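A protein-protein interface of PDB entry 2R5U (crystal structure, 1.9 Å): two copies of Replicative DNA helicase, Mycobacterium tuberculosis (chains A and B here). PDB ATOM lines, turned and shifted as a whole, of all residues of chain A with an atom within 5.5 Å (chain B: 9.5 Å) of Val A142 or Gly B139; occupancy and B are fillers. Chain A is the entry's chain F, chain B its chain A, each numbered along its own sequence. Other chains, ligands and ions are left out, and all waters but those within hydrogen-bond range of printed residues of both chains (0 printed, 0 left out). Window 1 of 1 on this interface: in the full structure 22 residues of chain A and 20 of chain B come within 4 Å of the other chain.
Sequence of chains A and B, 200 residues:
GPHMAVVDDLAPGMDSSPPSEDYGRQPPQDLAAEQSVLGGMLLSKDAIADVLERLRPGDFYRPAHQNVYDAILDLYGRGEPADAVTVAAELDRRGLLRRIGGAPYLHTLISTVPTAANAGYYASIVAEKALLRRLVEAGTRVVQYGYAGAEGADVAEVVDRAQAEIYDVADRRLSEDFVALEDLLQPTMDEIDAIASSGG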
ATOM      1  N   GLU A 137     -15.555  -9.787  12.902  1.00  0.00           N
ATOM      2  CA  GLU A 137     -16.137  -8.524  12.469  1.00  0.00           C
ATOM      3  C   GLU A 137     -17.389  -8.197  13.288  1.00  0.00           C
ATOM      4  O   GLU A 137     -17.557  -7.054  13.722  1.00  0.00           O
ATOM      5  CB  GLU A 137     -16.481  -8.557  10.969  1.00  0.00           C
ATOM      6  N   ALA A 138     -18.252  -9.194  13.500  1.00  0.00           N
ATOM      7  CA  ALA A 138     -19.474  -9.003  14.287  1.00  0.00           C
ATOM      8  C   ALA A 138     -19.159  -8.668  15.761  1.00  0.00           C
ATOM      9  O   ALA A 138     -19.712  -7.719  16.311  1.00  0.00           O
ATOM     10  CB  ALA A 138     -20.371 -10.227  14.197  1.00  0.00           C
ATOM     11  N   GLY A 139     -18.258  -9.444  16.367  1.00  0.00           N
ATOM     12  CA  GLY A 139     -17.811  -9.241  17.747  1.00  0.00           C
ATOM     13  C   GLY A 139     -17.261  -7.841  17.922  1.00  0.00           C
ATOM     14  O   GLY A 139     -17.623  -7.140  18.869  1.00  0.00           O
ATOM     15  N   THR A 140     -16.390  -7.439  16.997  1.00  0.00           N
ATOM     16  CA  THR A 140     -15.812  -6.092  16.975  1.00  0.00           C
ATOM     17  C   THR A 140     -16.880  -4.979  16.901  1.00  0.00           C
ATOM     18  O   THR A 140     -16.774  -3.947  17.601  1.00  0.00           O
ATOM     19  CB  THR A 140     -14.799  -5.952  15.821  1.00  0.00           C
ATOM     20  OG1 THR A 140     -13.726  -6.879  16.022  1.00  0.00           O
ATOM     21  CG2 THR A 140     -14.237  -4.534  15.753  1.00  0.00           C
ATOM     22  N   ARG A 141     -17.903  -5.194  16.074  1.00  0.00           N
ATOM     23  CA  ARG A 141     -19.028  -4.261  15.973  1.00  0.00           C
ATOM     24  C   ARG A 141     -19.805  -4.123  17.293  1.00  0.00           C
ATOM     25  O   ARG A 141     -20.151  -3.004  17.709  1.00  0.00           O
ATOM     26  CB  ARG A 141     -19.968  -4.666  14.839  1.00  0.00           C
ATOM     27  N   VAL A 142     -20.068  -5.262  17.938  1.00  0.00           N
ATOM     28  CA  VAL A 142     -20.783  -5.330  19.220  1.00  0.00           C
ATOM     29  C   VAL A 142     -20.054  -4.532  20.309  1.00  0.00           C
ATOM     30  O   VAL A 142     -20.678  -3.782  21.053  1.00  0.00           O
ATOM     31  CB  VAL A 142     -20.953  -6.807  19.670  1.00  0.00           C
ATOM     32  CG1 VAL A 142     -21.439  -6.914  21.128  1.00  0.00           C
ATOM     33  CG2 VAL A 142     -21.887  -7.551  18.726  1.00  0.00           C
ATOM     34  N   VAL A 143     -18.737  -4.696  20.376  1.00  0.00           N
ATOM     35  CA  VAL A 143     -17.887  -3.942  21.295  1.00  0.00           C
ATOM     36  C   VAL A 143     -18.065  -2.434  21.076  1.00  0.00           C
ATOM     37  O   VAL A 143     -18.143  -1.664  22.055  1.00  0.00           O
ATOM     38  CB  VAL A 143     -16.399  -4.334  21.151  1.00  0.00           C
ATOM     39  CG1 VAL A 143     -15.495  -3.372  21.929  1.00  0.00           C
ATOM     40  CG2 VAL A 143     -16.177  -5.744  21.620  1.00  0.00           C
ATOM     41  N   GLN A 144     -18.128  -2.022  19.804  1.00  0.00           N
ATOM     42  CA  GLN A 144     -18.319  -0.614  19.446  1.00  0.00           C
ATOM     43  C   GLN A 144     -19.684  -0.089  19.871  1.00  0.00           C
ATOM     44  O   GLN A 144     -19.790   1.051  20.309  1.00  0.00           O
ATOM     45  CB  GLN A 144     -18.113  -0.382  17.941  1.00  0.00           C
ATOM     46  CG  GLN A 144     -16.654  -0.432  17.501  1.00  0.00           C
ATOM     47  CD  GLN A 144     -16.467  -0.134  16.009  1.00  0.00           C
ATOM     48  OE1 GLN A 144     -17.274  -0.553  15.156  1.00  0.00           O
ATOM     49  NE2 GLN A 144     -15.400   0.594  15.689  1.00  0.00           N
ATOM     50  N   TYR A 145     -20.716  -0.925  19.745  1.00  0.00           N
ATOM     51  CA  TYR A 145     -22.070  -0.569  20.174  1.00  0.00           C
ATOM     52  C   TYR A 145     -22.124  -0.369  21.693  1.00  0.00           C
ATOM     53  O   TYR A 145     -22.737   0.591  22.188  1.00  0.00           O
ATOM     54  CB  TYR A 145     -23.094  -1.640  19.753  1.00  0.00           C
ATOM     55  CG  TYR A 145     -23.316  -1.785  18.257  1.00  0.00           C
ATOM     56  CD1 TYR A 145     -23.961  -2.915  17.742  1.00  0.00           C
ATOM     57  CD2 TYR A 145     -22.876  -0.810  17.357  1.00  0.00           C
ATOM     58  CE1 TYR A 145     -24.174  -3.068  16.383  1.00  0.00           C
ATOM     59  CE2 TYR A 145     -23.082  -0.955  15.983  1.00  0.00           C
ATOM     60  CZ  TYR A 145     -23.733  -2.088  15.508  1.00  0.00           C
ATOM     61  OH  TYR A 145     -23.942  -2.235  14.158  1.00  0.00           O
ATOM     62  N   GLY A 146     -21.479  -1.282  22.415  1.00  0.00           N
ATOM     63  CA  GLY A 146     -21.379  -1.216  23.867  1.00  0.00           C
ATOM     64  C   GLY A 146     -20.751   0.073  24.359  1.00  0.00           C
ATOM     65  O   GLY A 146     -21.198   0.644  25.358  1.00  0.00           O
ATOM     66  N   TYR A 147     -19.709   0.530  23.669  1.00  0.00           N
ATOM     67  CA  TYR A 147     -19.092   1.822  23.977  1.00  0.00           C
ATOM     68  C   TYR A 147     -19.922   3.028  23.536  1.00  0.00           C
ATOM     69  O   TYR A 147     -19.874   4.083  24.173  1.00  0.00           O
ATOM     70  CB  TYR A 147     -17.655   1.901  23.441  1.00  0.00           C
ATOM     71  CG  TYR A 147     -16.695   1.099  24.281  1.00  0.00           C
ATOM     72  CD1 TYR A 147     -16.000   0.023  23.745  1.00  0.00           C
ATOM     73  CD2 TYR A 147     -16.510   1.397  25.634  1.00  0.00           C
ATOM     74  CE1 TYR A 147     -15.136  -0.726  24.524  1.00  0.00           C
ATOM     75  CE2 TYR A 147     -15.647   0.660  26.420  1.00  0.00           C
ATOM     76  CZ  TYR A 147     -14.963  -0.398  25.865  1.00  0.00           C
ATOM     77  OH  TYR A 147     -14.101  -1.131  26.652  1.00  0.00           O
ATOM     78  N   ALA A 162     -26.803  -4.977  18.334  1.00  0.00           N
ATOM     79  CA  ALA A 162     -25.737  -5.914  18.671  1.00  0.00           C
ATOM     80  C   ALA A 162     -26.170  -7.356  18.418  1.00  0.00           C
ATOM     81  O   ALA A 162     -25.385  -8.170  17.931  1.00  0.00           O
ATOM     82  CB  ALA A 162     -25.279  -5.719  20.108  1.00  0.00           C
ATOM     83  N   GLU A 165     -26.504  -8.033  14.567  1.00  0.00           N
ATOM     84  CA  GLU A 165     -25.154  -8.293  14.077  1.00  0.00           C
ATOM     85  C   GLU A 165     -24.699  -9.750  14.233  1.00  0.00           C
ATOM     86  O   GLU A 165     -24.101 -10.308  13.316  1.00  0.00           O
ATOM     87  CB  GLU A 165     -24.164  -7.348  14.778  1.00  0.00           C
ATOM     88  CG  GLU A 165     -22.773  -7.271  14.151  1.00  0.00           C
ATOM     89  CD  GLU A 165     -22.717  -6.431  12.871  1.00  0.00           C
ATOM     90  OE1 GLU A 165     -21.706  -6.538  12.143  1.00  0.00           O
ATOM     91  OE2 GLU A 165     -23.665  -5.664  12.593  1.00  0.00           O
ATOM     92  N   ILE A 166     -24.971 -10.355  15.390  1.00  0.00           N
ATOM     93  CA  ILE A 166     -24.478 -11.708  15.694  1.00  0.00           C
ATOM     94  C   ILE A 166     -25.362 -12.807  15.102  1.00  0.00           C
ATOM     95  O   ILE A 166     -24.854 -13.822  14.641  1.00  0.00           O
ATOM     96  CB  ILE A 166     -24.233 -11.942  17.223  1.00  0.00           C
ATOM     97  CG1 ILE A 166     -23.248 -10.898  17.782  1.00  0.00           C
ATOM     98  CG2 ILE A 166     -23.704 -13.358  17.505  1.00  0.00           C
ATOM     99  CD1 ILE A 166     -21.763 -11.152  17.460  1.00  0.00           C
ATOM    100  N   PRO B  28     -17.741   0.076  30.350  1.00  0.00           N
ATOM    101  CA  PRO B  28     -18.896   0.884  30.750  1.00  0.00           C
ATOM    102  C   PRO B  28     -19.186   0.733  32.241  1.00  0.00           C
ATOM    103  O   PRO B  28     -19.259  -0.393  32.747  1.00  0.00           O
ATOM    104  CB  PRO B  28     -20.023   0.304  29.908  1.00  0.00           C
ATOM    105  CG  PRO B  28     -19.285  -0.171  28.645  1.00  0.00           C
ATOM    106  CD  PRO B  28     -18.063  -0.801  29.206  1.00  0.00           C
ATOM    107  N   LEU B 131     -25.342  -3.828  31.800  1.00  0.00           N
ATOM    108  CA  LEU B 131     -25.807  -4.400  30.514  1.00  0.00           C
ATOM    109  C   LEU B 131     -24.791  -4.064  29.419  1.00  0.00           C
ATOM    110  O   LEU B 131     -24.306  -4.955  28.738  1.00  0.00           O
ATOM    111  CB  LEU B 131     -27.204  -3.869  30.158  1.00  0.00           C
ATOM    112  CG  LEU B 131     -28.058  -4.468  29.029  1.00  0.00           C
ATOM    113  CD1 LEU B 131     -28.369  -5.963  29.284  1.00  0.00           C
ATOM    114  CD2 LEU B 131     -29.355  -3.648  28.904  1.00  0.00           C
ATOM    115  N   LEU B 132     -24.444  -2.786  29.289  1.00  0.00           N
ATOM    116  CA  LEU B 132     -23.454  -2.324  28.311  1.00  0.00           C
ATOM    117  C   LEU B 132     -22.084  -2.984  28.469  1.00  0.00           C
ATOM    118  O   LEU B 132     -21.458  -3.373  27.479  1.00  0.00           O
ATOM    119  CB  LEU B 132     -23.317  -0.798  28.344  1.00  0.00           C
ATOM    120  CG  LEU B 132     -24.522   0.006  27.856  1.00  0.00           C
ATOM    121  CD1 LEU B 132     -24.285   1.463  28.177  1.00  0.00           C
ATOM    122  CD2 LEU B 132     -24.749  -0.189  26.340  1.00  0.00           C
ATOM    123  N   ARG B 133     -21.628  -3.111  29.707  1.00  0.00           N
ATOM    124  CA  ARG B 133     -20.353  -3.750  30.010  1.00  0.00           C
ATOM    125  C   ARG B 133     -20.323  -5.235  29.651  1.00  0.00           C
ATOM    126  O   ARG B 133     -19.320  -5.720  29.109  1.00  0.00           O
ATOM    127  CB  ARG B 133     -20.004  -3.572  31.494  1.00  0.00           C
ATOM    128  CG  ARG B 133     -18.611  -4.033  31.865  1.00  0.00           C
ATOM    129  CD  ARG B 133     -18.214  -3.528  33.239  1.00  0.00           C
ATOM    130  NE  ARG B 133     -18.986  -4.188  34.292  1.00  0.00           N
ATOM    131  CZ  ARG B 133     -19.987  -3.635  34.982  1.00  0.00           C
ATOM    132  NH1 ARG B 133     -20.381  -2.384  34.769  1.00  0.00           N
ATOM    133  NH2 ARG B 133     -20.601  -4.360  35.900  1.00  0.00           N
ATOM    134  N   ARG B 134     -21.392  -5.961  29.988  1.00  0.00           N
ATOM    135  CA  ARG B 134     -21.523  -7.360  29.575  1.00  0.00           C
ATOM    136  C   ARG B 134     -21.656  -7.479  28.033  1.00  0.00           C
ATOM    137  O   ARG B 134     -21.268  -8.490  27.448  1.00  0.00           O
ATOM    138  CB  ARG B 134     -22.738  -8.011  30.220  1.00  0.00           C
ATOM    139  CG  ARG B 134     -22.643  -8.171  31.724  1.00  0.00           C
ATOM    140  CD  ARG B 134     -23.714  -9.124  32.263  1.00  0.00           C
ATOM    141  NE  ARG B 134     -25.100  -8.656  32.093  1.00  0.00           N
ATOM    142  CZ  ARG B 134     -25.745  -7.852  32.945  1.00  0.00           C
ATOM    143  NH1 ARG B 134     -25.123  -7.362  34.010  1.00  0.00           N
ATOM    144  NH2 ARG B 134     -27.002  -7.495  32.707  1.00  0.00           N
ATOM    145  N   LEU B 135     -22.240  -6.465  27.395  1.00  0.00           N
ATOM    146  CA  LEU B 135     -22.301  -6.443  25.928  1.00  0.00           C
ATOM    147  C   LEU B 135     -20.876  -6.353  25.349  1.00  0.00           C
ATOM    148  O   LEU B 135     -20.524  -7.106  24.444  1.00  0.00           O
ATOM    149  CB  LEU B 135     -23.188  -5.312  25.420  1.00  0.00           C
ATOM    150  CG  LEU B 135     -23.536  -5.304  23.925  1.00  0.00           C
ATOM    151  CD1 LEU B 135     -24.318  -6.564  23.528  1.00  0.00           C
ATOM    152  CD2 LEU B 135     -24.295  -4.020  23.539  1.00  0.00           C
ATOM    153  N   VAL B 136     -20.064  -5.465  25.918  1.00  0.00           N
ATOM    154  CA  VAL B 136     -18.662  -5.312  25.547  1.00  0.00           C
ATOM    155  C   VAL B 136     -17.855  -6.581  25.823  1.00  0.00           C
ATOM    156  O   VAL B 136     -17.041  -6.990  24.969  1.00  0.00           O
ATOM    157  CB  VAL B 136     -18.030  -4.056  26.219  1.00  0.00           C
ATOM    158  CG1 VAL B 136     -16.503  -4.077  26.149  1.00  0.00           C
ATOM    159  CG2 VAL B 136     -18.594  -2.788  25.594  1.00  0.00           C
ATOM    160  N   GLU B 137     -18.088  -7.215  26.977  1.00  0.00           N
ATOM    161  CA  GLU B 137     -17.396  -8.462  27.337  1.00  0.00           C
ATOM    162  C   GLU B 137     -17.766  -9.611  26.402  1.00  0.00           C
ATOM    163  O   GLU B 137     -16.887 -10.356  25.960  1.00  0.00           O
ATOM    164  CB  GLU B 137     -17.688  -8.883  28.783  1.00  0.00           C
ATOM    165  CG  GLU B 137     -16.898  -8.091  29.841  1.00  0.00           C
ATOM    166  CD  GLU B 137     -17.474  -8.244  31.261  1.00  0.00           C
ATOM    167  OE1 GLU B 137     -18.384  -9.088  31.486  1.00  0.00           O
ATOM    168  OE2 GLU B 137     -17.010  -7.502  32.147  1.00  0.00           O
ATOM    169  N   ALA B 138     -19.061  -9.759  26.131  1.00  0.00           N
ATOM    170  CA  ALA B 138     -19.562 -10.750  25.185  1.00  0.00           C
ATOM    171  C   ALA B 138     -18.985 -10.525  23.777  1.00  0.00           C
ATOM    172  O   ALA B 138     -18.591 -11.475  23.111  1.00  0.00           O
ATOM    173  CB  ALA B 138     -21.075 -10.721  25.139  1.00  0.00           C
ATOM    174  N   GLY B 139     -18.932  -9.267  23.349  1.00  0.00           N
ATOM    175  CA  GLY B 139     -18.401  -8.897  22.030  1.00  0.00           C
ATOM    176  C   GLY B 139     -16.937  -9.270  21.893  1.00  0.00           C
ATOM    177  O   GLY B 139     -16.525  -9.823  20.873  1.00  0.00           O
ATOM    178  N   THR B 140     -16.146  -8.978  22.925  1.00  0.00           N
ATOM    179  CA  THR B 140     -14.734  -9.364  22.924  1.00  0.00           C
ATOM    180  C   THR B 140     -14.565 -10.884  22.985  1.00  0.00           C
ATOM    181  O   THR B 140     -13.631 -11.421  22.384  1.00  0.00           O
ATOM    182  CB  THR B 140     -13.932  -8.732  24.064  1.00  0.00           C
ATOM    183  OG1 THR B 140     -14.272  -9.392  25.277  1.00  0.00           O
ATOM    184  CG2 THR B 140     -14.218  -7.256  24.193  1.00  0.00           C
ATOM    185  N   ARG B 141     -15.452 -11.568  23.711  1.00  0.00           N
ATOM    186  CA  ARG B 141     -15.466 -13.041  23.740  1.00  0.00           C
ATOM    187  C   ARG B 141     -15.803 -13.661  22.361  1.00  0.00           C
ATOM    188  O   ARG B 141     -15.191 -14.664  21.948  1.00  0.00           O
ATOM    189  CB  ARG B 141     -16.458 -13.547  24.793  1.00  0.00           C
ATOM    190  CG  ARG B 141     -16.497 -15.050  24.959  1.00  0.00           C
ATOM    191  CD  ARG B 141     -15.255 -15.529  25.695  1.00  0.00           C
ATOM    192  NE  ARG B 141     -15.043 -16.975  25.633  1.00  0.00           N
ATOM    193  CZ  ARG B 141     -14.400 -17.602  24.647  1.00  0.00           C
ATOM    194  NH1 ARG B 141     -14.256 -18.917  24.696  1.00  0.00           N
ATOM    195  NH2 ARG B 141     -13.917 -16.929  23.605  1.00  0.00           N
ATOM    196  N   VAL B 142     -16.790 -13.079  21.676  1.00  0.00           N
ATOM    197  CA  VAL B 142     -17.106 -13.471  20.289  1.00  0.00           C
ATOM    198  C   VAL B 142     -15.864 -13.321  19.384  1.00  0.00           C
ATOM    199  O   VAL B 142     -15.513 -14.255  18.660  1.00  0.00           O
ATOM    200  CB  VAL B 142     -18.350 -12.687  19.741  1.00  0.00           C
ATOM    201  CG1 VAL B 142     -18.532 -12.875  18.232  1.00  0.00           C
ATOM    202  CG2 VAL B 142     -19.629 -13.105  20.494  1.00  0.00           C
ATOM    203  N   VAL B 143     -15.196 -12.162  19.439  1.00  0.00           N
ATOM    204  CA  VAL B 143     -13.923 -11.963  18.727  1.00  0.00           C
ATOM    205  C   VAL B 143     -12.927 -13.098  19.017  1.00  0.00           C
ATOM    206  O   VAL B 143     -12.323 -13.639  18.089  1.00  0.00           O
ATOM    207  CB  VAL B 143     -13.269 -10.579  19.031  1.00  0.00           C
ATOM    208  CG1 VAL B 143     -11.806 -10.520  18.537  1.00  0.00           C
ATOM    209  CG2 VAL B 143     -14.093  -9.437  18.445  1.00  0.00           C
ATOM    210  N   GLN B 144     -12.789 -13.463  20.293  1.00  0.00           N
ATOM    211  CA  GLN B 144     -11.887 -14.535  20.769  1.00  0.00           C
ATOM    212  C   GLN B 144     -12.266 -15.901  20.169  1.00  0.00           C
ATOM    213  O   GLN B 144     -11.400 -16.721  19.821  1.00  0.00           O
ATOM    214  CB  GLN B 144     -11.972 -14.599  22.298  1.00  0.00           C
ATOM    215  CG  GLN B 144     -10.727 -14.991  23.058  1.00  0.00           C
ATOM    216  CD  GLN B 144     -10.756 -14.432  24.496  1.00  0.00           C
ATOM    217  OE1 GLN B 144     -11.665 -14.735  25.287  1.00  0.00           O
ATOM    218  NE2 GLN B 144      -9.769 -13.599  24.827  1.00  0.00           N
ATOM    219  N   TYR B 145     -13.566 -16.144  20.060  1.00  0.00           N
ATOM    220  CA  TYR B 145     -14.085 -17.311  19.355  1.00  0.00           C
ATOM    221  C   TYR B 145     -13.665 -17.338  17.862  1.00  0.00           C
ATOM    222  O   TYR B 145     -13.268 -18.382  17.334  1.00  0.00           O
ATOM    223  CB  TYR B 145     -15.614 -17.359  19.486  1.00  0.00           C
ATOM    224  CG  TYR B 145     -16.133 -18.136  20.686  1.00  0.00           C
ATOM    225  CD1 TYR B 145     -17.182 -17.637  21.473  1.00  0.00           C
ATOM    226  CD2 TYR B 145     -15.595 -19.387  21.019  1.00  0.00           C
ATOM    227  CE1 TYR B 145     -17.674 -18.367  22.572  1.00  0.00           C
ATOM    228  CE2 TYR B 145     -16.074 -20.116  22.104  1.00  0.00           C
ATOM    229  CZ  TYR B 145     -17.102 -19.607  22.882  1.00  0.00           C
ATOM    230  OH  TYR B 145     -17.553 -20.355  23.963  1.00  0.00           O
ATOM    231  N   GLY B 146     -13.754 -16.190  17.195  1.00  0.00           N
ATOM    232  CA  GLY B 146     -13.395 -16.075  15.777  1.00  0.00           C
ATOM    233  C   GLY B 146     -11.926 -16.408  15.567  1.00  0.00           C
ATOM    234  O   GLY B 146     -11.581 -17.223  14.701  1.00  0.00           O
ATOM    235  N   TYR B 147     -11.068 -15.794  16.383  1.00  0.00           N
ATOM    236  CA  TYR B 147      -9.623 -16.005  16.274  1.00  0.00           C
ATOM    237  C   TYR B 147      -9.155 -17.376  16.738  1.00  0.00           C
ATOM    238  O   TYR B 147      -8.142 -17.868  16.244  1.00  0.00           O
ATOM    239  CB  TYR B 147      -8.834 -14.913  17.005  1.00  0.00           C
ATOM    240  CG  TYR B 147      -8.804 -13.580  16.297  1.00  0.00           C
ATOM    241  CD1 TYR B 147      -9.159 -12.416  16.965  1.00  0.00           C
ATOM    242  CD2 TYR B 147      -8.409 -13.479  14.959  1.00  0.00           C
ATOM    243  CE1 TYR B 147      -9.136 -11.172  16.320  1.00  0.00           C
ATOM    244  CE2 TYR B 147      -8.379 -12.244  14.303  1.00  0.00           C
ATOM    245  CZ  TYR B 147      -8.746 -11.093  14.993  1.00  0.00           C
ATOM    246  OH  TYR B 147      -8.727  -9.868  14.367  1.00  0.00           O
ATOM    247  N   ALA B 162     -20.867 -18.492  20.149  1.00  0.00           N
ATOM    248  CA  ALA B 162     -20.764 -17.036  20.062  1.00  0.00           C
ATOM    249  C   ALA B 162     -22.156 -16.386  20.082  1.00  0.00           C
ATOM    250  O   ALA B 162     -22.333 -15.311  20.660  1.00  0.00           O
ATOM    251  CB  ALA B 162     -19.986 -16.615  18.839  1.00  0.00           C
ATOM    252  N   GLN B 163     -23.134 -17.044  19.467  1.00  0.00           N
ATOM    253  CA  GLN B 163     -24.507 -16.531  19.473  1.00  0.00           C
ATOM    254  C   GLN B 163     -25.134 -16.580  20.882  1.00  0.00           C
ATOM    255  O   GLN B 163     -25.896 -15.682  21.253  1.00  0.00           O
ATOM    256  CB  GLN B 163     -25.369 -17.245  18.418  1.00  0.00           C
ATOM    257  CG  GLN B 163     -25.002 -16.806  16.982  1.00  0.00           C
ATOM    258  CD  GLN B 163     -25.607 -17.681  15.881  1.00  0.00           C
ATOM    259  OE1 GLN B 163     -25.964 -18.846  16.103  1.00  0.00           O
ATOM    260  NE2 GLN B 163     -25.690 -17.121  14.665  1.00  0.00           N
ATOM    261  N   ALA B 164     -24.789 -17.605  21.659  1.00  0.00           N
ATOM    262  CA  ALA B 164     -25.268 -17.737  23.043  1.00  0.00           C
ATOM    263  C   ALA B 164     -24.645 -16.666  23.967  1.00  0.00           C
ATOM    264  O   ALA B 164     -25.287 -16.198  24.911  1.00  0.00           O
ATOM    265  CB  ALA B 164     -24.993 -19.135  23.575  1.00  0.00           C
ATOM    266  N   GLU B 165     -23.393 -16.297  23.684  1.00  0.00           N
ATOM    267  CA  GLU B 165     -22.686 -15.233  24.403  1.00  0.00           C
ATOM    268  C   GLU B 165     -23.438 -13.917  24.361  1.00  0.00           C
ATOM    269  O   GLU B 165     -23.537 -13.205  25.365  1.00  0.00           O
ATOM    270  CB  GLU B 165     -21.297 -15.015  23.790  1.00  0.00           C
ATOM    271  CG  GLU B 165     -20.252 -15.955  24.316  1.00  0.00           C
ATOM    272  CD  GLU B 165     -19.973 -15.710  25.774  1.00  0.00           C
ATOM    273  OE1 GLU B 165     -19.906 -16.696  26.539  1.00  0.00           O
ATOM    274  OE2 GLU B 165     -19.838 -14.525  26.154  1.00  0.00           O
ATOM    275  N   ILE B 166     -23.961 -13.605  23.183  1.00  0.00           N
ATOM    276  CA  ILE B 166     -24.663 -12.364  22.948  1.00  0.00           C
ATOM    277  C   ILE B 166     -26.078 -12.496  23.521  1.00  0.00           C
ATOM    278  O   ILE B 166     -26.636 -11.525  24.050  1.00  0.00           O
ATOM    279  CB  ILE B 166     -24.614 -11.977  21.435  1.00  0.00           C
ATOM    280  CG1 ILE B 166     -23.152 -11.817  20.986  1.00  0.00           C
ATOM    281  CG2 ILE B 166     -25.390 -10.691  21.132  1.00  0.00           C
ATOM    282  CD1 ILE B 166     -22.396 -10.623  21.629  1.00  0.00           C
ATOM    283  N   TYR B 167     -26.636 -13.706  23.440  1.00  0.00           N
ATOM    284  CA  TYR B 167     -27.909 -14.003  24.093  1.00  0.00           C
ATOM    285  C   TYR B 167     -27.824 -13.764  25.606  1.00  0.00           C
ATOM    286  O   TYR B 167     -28.668 -13.076  26.163  1.00  0.00           O
ATOM    287  CB  TYR B 167     -28.377 -15.434  23.787  1.00  0.00           C
ATOM    288  N   VAL B 169     -26.329 -11.764  27.423  1.00  0.00           N
ATOM    289  CA  VAL B 169     -26.185 -10.378  27.873  1.00  0.00           C
ATOM    290  C   VAL B 169     -27.458  -9.874  28.568  1.00  0.00           C
ATOM    291  O   VAL B 169     -28.561  -9.940  28.016  1.00  0.00           O
ATOM    292  CB  VAL B 169     -25.802  -9.449  26.704  1.00  0.00           C
ATOM    293  CG1 VAL B 169     -25.689  -8.000  27.164  1.00  0.00           C
ATOM    294  CG2 VAL B 169     -24.497  -9.914  26.087  1.00  0.00           C
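The side-chain amide nitrogen (NE2) of Gln B163 lies within hydrogen-bond range of the backbone carbonyl oxygen (O) of Ile A166 (3.4 Å).
O of Pro B28 sits at hydrogen-bond distance from NH1 of Arg B133, 3.1 Å away. OG1 of Thr B140 is in hydrogen-bond range of O of Glu B137 (2.9 Å).
Among the printed residues, merely in contact across the chains: Ile A166 with Ile B166, Thr A140 with Val B143, Gly A139 with Gly B139, Val A142 with Leu B135, Val A143 with Thr B140, Gly A139 with Val B143, Val A143 with Gly B139, Gly A146 with Val B136, Ala A162 with Leu B135, Val A143 with Val B136, Gly A139 with Val B142, Val A142 with Gly B139, Ile A166 with Val B142, Gly A146 with Leu B132, Tyr A147 with Val B136, Val A142 with Ile B166, Gly A146 with Pro B28, Ile A166 with Ala B162 and Tyr A147 with Pro B28.
Ala A138 touches none of the printed residues of chain B. No residue of chain B comes within 4 Å of Arg A141. Of the printed residues of chain B, Ala A162 touches Leu B135 (3.7 Å). Printed residues of chain A within 4 Å of Val B136: Val A143, Gly A146 and Tyr A147. Ala B138 touches none of the printed residues of chain A. Of the printed residues of chain A, Gly B139 touches Gly A139 (3.4 Å), Val A142 (3.7 Å) and Val A143 (3.6 Å). Printed residues of chain A within 4 Å of Ile B166: Val A142 (3.9 Å) and Ile A166 (3.3 Å). The nearest printed residue of chain B that does not touch Val A142 is Val B136 (5.1 Å). The nearest residue of chain A that does not touch Gly B139 is Thr A140 (4.6 Å).
Printed residues of chain A that touch a printed residue of chain B: Gly A139, Thr A140, Val A142, Val A143, Gly A146, Tyr A147, Ala A162 and Ile A166. Hydrophobic or aromatic side chains of chain A that line the printed part of chain B: Val A142, Val A143, Tyr A147, Ala A162 and Ile A166. Hydrophobic or aromatic side chains of chain B that line the printed part of chain A: Pro B28, Leu B132, Leu B135, Val B136, Val B142, Val B143 and Ile B166. Among the printed residues, 20 pairs touch across the chains. Among the printed residues, no Asp or Glu carboxylate lies within 4 Å of a Lys or Arg side-chain nitrogen of the other chain.
Gly A139 touches its own counterpart, Gly B139. Gly A139 touches Val B143, and with the chains exchanged Val A143 touches Gly B139. Val A142 touches Ile B166, and with the chains exchanged Ile A166 touches Val B142. Ile B166 touches its own counterpart, Ile A166. 14 positions are printed for both chains. Of the 20 pairs that touch across the chains among the printed residues, 10 have their exchanged pair printed and touching as well.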
